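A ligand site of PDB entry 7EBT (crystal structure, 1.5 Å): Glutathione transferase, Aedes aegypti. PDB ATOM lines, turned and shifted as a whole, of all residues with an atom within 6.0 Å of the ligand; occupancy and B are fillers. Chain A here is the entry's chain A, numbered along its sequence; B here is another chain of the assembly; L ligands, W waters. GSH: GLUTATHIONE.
An oxygen (O2) of the ligand lies within hydrogen-bond range of the backbone NH of Val 64 (2.9 Å).
N of Ser 77 sits at hydrogen-bond distance from O12 of the ligand (2.8 Å).
The side-chain amide oxygen (OD1) of Asn 113 lies within hydrogen-bond range of a nitrogen (N1) of the ligand, 2.8 Å away.
The side-chain carboxylate (OD2) of Asp 76 is in salt-bridge range of a nitrogen (N1) of the ligand (2.8 Å).
A ring nitrogen (ND1) of His 62 lies within hydrogen-bond range of an oxygen (O32) of the ligand, at 2.8 Å.
A ring nitrogen (ND1) of His 78 lies within hydrogen-bond range of an oxygen (O11) of the ligand, 3.4 Å away.
A sulfur (SG2) of the ligand sits close to the side-chain hydroxyl of Ser 19 (3.2 Å).
The side-chain hydroxyl (OG) of Ser 77 lies within hydrogen-bond range of an oxygen (O11) of the ligand (2.7 Å).
N2 of the ligand is in hydrogen-bond range of O of Val 64 (3.0 Å).
Merely in contact with the ligand: Ala 63, His 50, Pro 65, Pro 21, Phe 117, Leu 45 and Ala 114 of chain B.
Hydrophobic or aromatic side chains within 4 Å of the ligand: Pro 21, Leu 45, His 50, His 62, Ala 63, Val 64, Pro 65, His 78, Phe 117 and Ala 114 of chain B.
14 residues have an atom within 4 Å of the ligand: Ser 19, Pro 21, Leu 45, His 50, His 62, Ala 63, Val 64, Pro 65, Asp 76, Ser 77, His 78, Asn 113, Phe 117 and Ala 114 of chain B.
The nearest printed residue that does not touch the ligand is Pro 20 (4.1 Å).
ND1 of His 78 lies within hydrogen-bond range of OG of Ser 77 (3.2 Å).
The side-chain carboxylate (OD1) of Asp 76 sits at hydrogen-bond distance from a ring nitrogen (ND1) of His 78 (2.8 Å).
The side-chain amide nitrogen (ND2) of Asn 113 is in hydrogen-bond range of the side-chain carboxylate (OD2) of Asp 76 (3.1 Å).
The backbone carbonyl oxygen (O) of Asn 113 sits at hydrogen-bond distance from the side-chain amide nitrogen (NE2) of Gln 118 (2.9 Å).
The side-chain amide nitrogen (NE2) of Gln 118 sits at hydrogen-bond distance from the backbone carbonyl oxygen (O) of Ala 114 of chain B, at 3.5 Å.
The side-chain amide oxygen (OD1) of Asn 113 sits close to a ring nitrogen (ND1) of His 78 (3.3 Å).
Water W3 lies within hydrogen-bond range of the backbone carbonyl oxygen (O) of Pro 65 (2.8 Å), an oxygen (O12) of the ligand (2.9 Å) and the backbone carbonyl oxygen (O) of Val 64 (3.4 Å).
Water W4 lies within hydrogen-bond range of N1 of the ligand (3.0 Å), NE2 of Gln 118 (3.2 Å) and O of Ala 114 of chain B (3.3 Å).
Water W2 lies within hydrogen-bond range of NE2 of His 50 (2.9 Å) and O32 of the ligand (3.3 Å).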
ATOM      1  N   SER A  19      11.517  -7.705  17.696  1.00  0.00           N
ATOM      2  CA  SER A  19      11.312  -6.280  17.975  1.00  0.00           C
ATOM      3  C   SER A  19      12.267  -5.780  19.061  1.00  0.00           C
ATOM      4  O   SER A  19      12.274  -6.350  20.153  1.00  0.00           O
ATOM      5  CB  SER A  19       9.885  -6.050  18.437  1.00  0.00           C
ATOM      6  OG  SER A  19       9.745  -4.838  19.162  1.00  0.00           O
ATOM      7  N   PRO A  20      13.026  -4.705  18.827  1.00  0.00           N
ATOM      8  CA  PRO A  20      13.882  -4.174  19.914  1.00  0.00           C
ATOM      9  C   PRO A  20      13.076  -3.732  21.127  1.00  0.00           C
ATOM     10  O   PRO A  20      13.462  -4.055  22.261  1.00  0.00           O
ATOM     11  CB  PRO A  20      14.626  -2.994  19.254  1.00  0.00           C
ATOM     12  CG  PRO A  20      14.474  -3.185  17.783  1.00  0.00           C
ATOM     13  CD  PRO A  20      13.278  -4.062  17.528  1.00  0.00           C
ATOM     14  N   PRO A  21      11.937  -3.027  20.967  1.00  0.00           N
ATOM     15  CA  PRO A  21      11.129  -2.728  22.163  1.00  0.00           C
ATOM     16  C   PRO A  21      10.784  -3.959  22.988  1.00  0.00           C
ATOM     17  O   PRO A  21      10.866  -3.933  24.218  1.00  0.00           O
ATOM     18  CB  PRO A  21       9.868  -2.065  21.585  1.00  0.00           C
ATOM     19  CG  PRO A  21      10.380  -1.383  20.354  1.00  0.00           C
ATOM     20  CD  PRO A  21      11.415  -2.326  19.771  1.00  0.00           C
ATOM     21  N   LEU A  45       4.648 -10.806  14.282  1.00  0.00           N
ATOM     22  CA  LEU A  45       4.479  -9.672  13.376  1.00  0.00           C
ATOM     23  C   LEU A  45       4.514 -10.092  11.904  1.00  0.00           C
ATOM     24  O   LEU A  45       3.697  -9.622  11.107  1.00  0.00           O
ATOM     25  CB  LEU A  45       5.568  -8.622  13.647  1.00  0.00           C
ATOM     26  CG  LEU A  45       5.518  -8.032  15.060  1.00  0.00           C
ATOM     27  CD1 LEU A  45       6.662  -7.042  15.236  1.00  0.00           C
ATOM     28  CD2 LEU A  45       4.180  -7.337  15.258  1.00  0.00           C
ATOM     29  N   HIS A  50      -0.590  -9.204  14.823  1.00  0.00           N
ATOM     30  CA  HIS A  50      -0.866  -7.950  15.503  1.00  0.00           C
ATOM     31  C   HIS A  50      -2.015  -7.193  14.869  1.00  0.00           C
ATOM     32  O   HIS A  50      -2.425  -6.153  15.394  1.00  0.00           O
ATOM     33  CB  HIS A  50       0.383  -7.057  15.486  1.00  0.00           C
ATOM     34  CG  HIS A  50       0.894  -6.760  14.115  1.00  0.00           C
ATOM     35  ND1 HIS A  50       1.259  -7.743  13.220  1.00  0.00           N
ATOM     36  CD2 HIS A  50       1.072  -5.580  13.467  1.00  0.00           C
ATOM     37  CE1 HIS A  50       1.659  -7.190  12.097  1.00  0.00           C
ATOM     38  NE2 HIS A  50       1.557  -5.874  12.216  1.00  0.00           N
ATOM     39  N   LEU A  51      -2.557  -7.677  13.743  1.00  0.00           N
ATOM     40  CA  LEU A  51      -3.674  -7.021  13.093  1.00  0.00           C
ATOM     41  C   LEU A  51      -4.996  -7.732  13.325  1.00  0.00           C
ATOM     42  O   LEU A  51      -6.030  -7.283  12.810  1.00  0.00           O
ATOM     43  CB  LEU A  51      -3.395  -6.867  11.588  1.00  0.00           C
ATOM     44  CG  LEU A  51      -2.118  -6.060  11.320  1.00  0.00           C
ATOM     45  CD1 LEU A  51      -1.869  -6.021   9.819  1.00  0.00           C
ATOM     46  CD2 LEU A  51      -2.265  -4.645  11.882  1.00  0.00           C
ATOM     47  N   LEU A  61      -2.730   0.828  18.585  1.00  0.00           N
ATOM     48  CA  LEU A  61      -1.481   1.015  17.860  1.00  0.00           C
ATOM     49  C   LEU A  61      -1.043  -0.252  17.132  1.00  0.00           C
ATOM     50  O   LEU A  61      -0.068  -0.219  16.373  1.00  0.00           O
ATOM     51  CB  LEU A  61      -0.393   1.480  18.842  1.00  0.00           C
ATOM     52  CG  LEU A  61      -0.653   2.843  19.479  1.00  0.00           C
ATOM     53  CD1 LEU A  61       0.211   3.004  20.729  1.00  0.00           C
ATOM     54  CD2 LEU A  61      -0.367   3.930  18.451  1.00  0.00           C
ATOM     55  N   HIS A  62      -1.734  -1.374  17.381  1.00  0.00           N
ATOM     56  CA  HIS A  62      -1.419  -2.671  16.772  1.00  0.00           C
ATOM     57  C   HIS A  62       0.083  -2.952  16.763  1.00  0.00           C
ATOM     58  O   HIS A  62       0.697  -3.263  15.732  1.00  0.00           O
ATOM     59  CB  HIS A  62      -2.038  -2.824  15.363  1.00  0.00           C
ATOM     60  CG  HIS A  62      -1.718  -1.703  14.421  1.00  0.00           C
ATOM     61  ND1 HIS A  62      -0.529  -1.612  13.743  1.00  0.00           N
ATOM     62  CD2 HIS A  62      -2.463  -0.641  14.025  1.00  0.00           C
ATOM     63  CE1 HIS A  62      -0.542  -0.532  12.976  1.00  0.00           C
ATOM     64  NE2 HIS A  62      -1.705   0.079  13.133  1.00  0.00           N
ATOM     65  N   ALA A  63       0.689  -2.844  17.944  1.00  0.00           N
ATOM     66  CA  ALA A  63       2.135  -2.975  18.062  1.00  0.00           C
ATOM     67  C   ALA A  63       2.488  -3.786  19.298  1.00  0.00           C
ATOM     68  O   ALA A  63       1.719  -3.856  20.261  1.00  0.00           O
ATOM     69  CB  ALA A  63       2.818  -1.606  18.149  1.00  0.00           C
ATOM     70  N   VAL A  64       3.688  -4.368  19.286  1.00  0.00           N
ATOM     71  CA  VAL A  64       4.194  -5.118  20.439  1.00  0.00           C
ATOM     72  C   VAL A  64       5.403  -4.363  21.003  1.00  0.00           C
ATOM     73  O   VAL A  64       6.159  -3.723  20.251  1.00  0.00           O
ATOM     74  CB  VAL A  64       4.577  -6.555  20.064  1.00  0.00           C
ATOM     75  CG1 VAL A  64       3.286  -7.373  19.748  1.00  0.00           C
ATOM     76  CG2 VAL A  64       5.593  -6.584  18.923  1.00  0.00           C
ATOM     77  N   PRO A  65       5.660  -4.446  22.302  1.00  0.00           N
ATOM     78  CA  PRO A  65       4.960  -5.231  23.315  1.00  0.00           C
ATOM     79  C   PRO A  65       3.737  -4.569  23.936  1.00  0.00           C
ATOM     80  O   PRO A  65       3.553  -3.364  23.911  1.00  0.00           O
ATOM     81  CB  PRO A  65       6.040  -5.436  24.380  1.00  0.00           C
ATOM     82  CG  PRO A  65       6.813  -4.131  24.347  1.00  0.00           C
ATOM     83  CD  PRO A  65       6.855  -3.773  22.862  1.00  0.00           C
ATOM     84  N   THR A  75       0.916  -0.194  26.695  1.00  0.00           N
ATOM     85  CA  THR A  75       1.116  -0.316  25.255  1.00  0.00           C
ATOM     86  C   THR A  75       2.372   0.404  24.803  1.00  0.00           C
ATOM     87  O   THR A  75       2.440   0.953  23.708  1.00  0.00           O
ATOM     88  CB  THR A  75      -0.118   0.169  24.486  1.00  0.00           C
ATOM     89  OG1 THR A  75      -0.420   1.540  24.805  1.00  0.00           O
ATOM     90  CG2 THR A  75      -1.326  -0.692  24.855  1.00  0.00           C
ATOM     91  N   ASP A  76       3.398   0.412  25.658  1.00  0.00           N
ATOM     92  CA  ASP A  76       4.722   0.917  25.316  1.00  0.00           C
ATOM     93  C   ASP A  76       5.708   0.196  26.202  1.00  0.00           C
ATOM     94  O   ASP A  76       5.523   0.177  27.419  1.00  0.00           O
ATOM     95  CB  ASP A  76       4.821   2.435  25.488  1.00  0.00           C
ATOM     96  CG  ASP A  76       6.058   3.020  24.824  1.00  0.00           C
ATOM     97  OD1 ASP A  76       7.180   2.678  25.304  1.00  0.00           O
ATOM     98  OD2 ASP A  76       5.931   3.740  23.801  1.00  0.00           O
ATOM     99  N   SER A  77       6.750  -0.379  25.579  1.00  0.00           N
ATOM    100  CA  SER A  77       7.791  -1.108  26.290  1.00  0.00           C
ATOM    101  C   SER A  77       8.360  -0.310  27.464  1.00  0.00           C
ATOM    102  O   SER A  77       8.683  -0.891  28.510  1.00  0.00           O
ATOM    103  CB  SER A  77       8.913  -1.488  25.326  1.00  0.00           C
ATOM    104  OG  SER A  77       9.659  -0.350  24.869  1.00  0.00           O
ATOM    105  N   HIS A  78       8.488   1.015  27.300  1.00  0.00           N
ATOM    106  CA  HIS A  78       9.126   1.810  28.338  1.00  0.00           C
ATOM    107  C   HIS A  78       8.223   1.950  29.554  1.00  0.00           C
ATOM    108  O   HIS A  78       8.722   1.896  30.690  1.00  0.00           O
ATOM    109  CB  HIS A  78       9.554   3.152  27.735  1.00  0.00           C
ATOM    110  CG  HIS A  78      10.469   2.984  26.546  1.00  0.00           C
ATOM    111  ND1 HIS A  78       9.990   2.825  25.258  1.00  0.00           N
ATOM    112  CD2 HIS A  78      11.811   2.837  26.464  1.00  0.00           C
ATOM    113  CE1 HIS A  78      11.007   2.627  24.433  1.00  0.00           C
ATOM    114  NE2 HIS A  78      12.123   2.646  25.135  1.00  0.00           N
ATOM    115  N   ASN A 113      13.171   5.761  23.566  1.00  0.00           N
ATOM    116  CA  ASN A 113      11.893   5.730  22.867  1.00  0.00           C
ATOM    117  C   ASN A 113      11.812   6.825  21.808  1.00  0.00           C
ATOM    118  O   ASN A 113      11.348   6.580  20.683  1.00  0.00           O
ATOM    119  CB  ASN A 113      10.748   5.884  23.873  1.00  0.00           C
ATOM    120  CG  ASN A 113       9.469   5.272  23.397  1.00  0.00           C
ATOM    121  OD1 ASN A 113       9.453   4.493  22.443  1.00  0.00           O
ATOM    122  ND2 ASN A 113       8.395   5.596  24.080  1.00  0.00           N
ATOM    123  N   PHE A 117      15.429   4.689  19.289  1.00  0.00           N
ATOM    124  CA  PHE A 117      14.534   3.755  18.615  1.00  0.00           C
ATOM    125  C   PHE A 117      13.885   4.388  17.397  1.00  0.00           C
ATOM    126  O   PHE A 117      13.783   3.761  16.337  1.00  0.00           O
ATOM    127  CB  PHE A 117      13.465   3.219  19.575  1.00  0.00           C
ATOM    128  CG  PHE A 117      12.397   2.404  18.876  1.00  0.00           C
ATOM    129  CD1 PHE A 117      12.713   1.217  18.259  1.00  0.00           C
ATOM    130  CD2 PHE A 117      11.089   2.874  18.778  1.00  0.00           C
ATOM    131  CE1 PHE A 117      11.732   0.476  17.578  1.00  0.00           C
ATOM    132  CE2 PHE A 117      10.117   2.142  18.092  1.00  0.00           C
ATOM    133  CZ  PHE A 117      10.452   0.941  17.504  1.00  0.00           C
ATOM    134  N   GLN A 118      13.454   5.660  17.511  1.00  0.00           N
ATOM    135  CA  GLN A 118      12.809   6.314  16.381  1.00  0.00           C
ATOM    136  C   GLN A 118      13.732   6.337  15.172  1.00  0.00           C
ATOM    137  O   GLN A 118      13.308   6.043  14.046  1.00  0.00           O
ATOM    138  CB  GLN A 118      12.391   7.739  16.730  1.00  0.00           C
ATOM    139  CG  GLN A 118      11.287   7.845  17.799  1.00  0.00           C
ATOM    140  CD  GLN A 118      10.059   7.018  17.482  1.00  0.00           C
ATOM    141  OE1 GLN A 118       9.586   6.999  16.333  1.00  0.00           O
ATOM    142  NE2 GLN A 118       9.535   6.334  18.490  1.00  0.00           N
ATOM    143  N   SER A 121      14.657   2.647  13.847  1.00  0.00           N
ATOM    144  CA  SER A 121      13.522   1.962  13.235  1.00  0.00           C
ATOM    145  C   SER A 121      13.275   2.451  11.813  1.00  0.00           C
ATOM    146  O   SER A 121      12.924   1.662  10.929  1.00  0.00           O
ATOM    147  CB  SER A 121      12.266   2.153  14.090  1.00  0.00           C
ATOM    148  OG  SER A 121      11.182   1.420  13.557  1.00  0.00           O
ATOM    149  N   CYS B 110       4.194   8.153  27.003  1.00  0.00           N
ATOM    150  CA  CYS B 110       4.917   7.447  25.950  1.00  0.00           C
ATOM    151  C   CYS B 110       4.196   7.563  24.612  1.00  0.00           C
ATOM    152  O   CYS B 110       4.832   7.736  23.569  1.00  0.00           O
ATOM    153  CB  CYS B 110       5.056   5.975  26.318  1.00  0.00           C
ATOM    154  SG  CYS B 110       6.140   5.603  27.686  1.00  0.00           S
ATOM    155  N   ALA B 114       6.373   9.093  21.648  1.00  0.00           N
ATOM    156  CA  ALA B 114       6.808   8.159  20.616  1.00  0.00           C
ATOM    157  C   ALA B 114       5.864   8.056  19.428  1.00  0.00           C
ATOM    158  O   ALA B 114       6.259   7.499  18.386  1.00  0.00           O
ATOM    159  CB  ALA B 114       6.987   6.760  21.212  1.00  0.00           C
ATOM    160  N   VAL B 115       4.633   8.571  19.537  1.00  0.00           N
ATOM    161  CA  VAL B 115       3.666   8.467  18.447  1.00  0.00           C
ATOM    162  C   VAL B 115       3.213   9.854  18.006  1.00  0.00           C
ATOM    163  O   VAL B 115       3.602  10.321  16.936  1.00  0.00           O
ATOM    164  CB  VAL B 115       2.469   7.585  18.836  1.00  0.00           C
ATOM    165  CG1 VAL B 115       1.540   7.455  17.646  1.00  0.00           C
ATOM    166  CG2 VAL B 115       2.969   6.206  19.297  1.00  0.00           C
HETATM  167  N1  GSH L   1       7.297   2.957  21.461  1.00  0.00           N
HETATM  168  CA1 GSH L   1       6.798   1.563  21.262  1.00  0.00           C
HETATM  169  C1  GSH L   1       7.370   0.656  22.375  1.00  0.00           C
HETATM  170  O11 GSH L   1       8.518   0.996  22.832  1.00  0.00           O
HETATM  171  O12 GSH L   1       6.741  -0.301  22.772  1.00  0.00           O
HETATM  172  CB1 GSH L   1       7.187   1.061  19.875  1.00  0.00           C
HETATM  173  CG1 GSH L   1       6.505  -0.281  19.584  1.00  0.00           C
HETATM  174  CD1 GSH L   1       6.645  -0.676  18.133  1.00  0.00           C
HETATM  175  OE1 GSH L   1       6.763   0.175  17.245  1.00  0.00           O
HETATM  176  N2  GSH L   1       6.641  -1.993  17.882  1.00  0.00           N
HETATM  177  CA2 GSH L   1       6.759  -2.495  16.523  1.00  0.00           C
HETATM  178  C2  GSH L   1       5.439  -3.098  16.030  1.00  0.00           C
HETATM  179  O2  GSH L   1       4.855  -3.935  16.698  1.00  0.00           O
HETATM  180  CB2 GSH L   1       7.872  -3.519  16.405  1.00  0.00           C
HETATM  181  SG2 GSH L   1       9.513  -2.836  16.677  1.00  0.00           S
HETATM  182  N3  GSH L   1       5.019  -2.668  14.841  1.00  0.00           N
HETATM  183  CA3 GSH L   1       3.789  -3.186  14.253  1.00  0.00           C
HETATM  184  C3  GSH L   1       3.075  -2.212  13.348  1.00  0.00           C
HETATM  185  O31 GSH L   1       3.735  -1.098  13.187  1.00  0.00           O
HETATM  186  O32 GSH L   1       1.993  -2.440  12.847  1.00  0.00           O
HETATM  187  O   HOH W   1       6.861   2.769  16.644  1.00  0.00           O
HETATM  188  O   HOH W   2       1.901  -4.106   9.987  1.00  0.00           O
HETATM  189  O   HOH W   3       4.271  -1.474  21.937  1.00  0.00           O
HETATM  190  O   HOH W   4       7.095   4.346  18.856  1.00  0.00           O
HETATM  191  O   HOH W   5       4.979   0.646  15.120  1.00  0.00           O
HETATM  192  O   HOH W   6       2.088   1.796  12.864  1.00  0.00           O
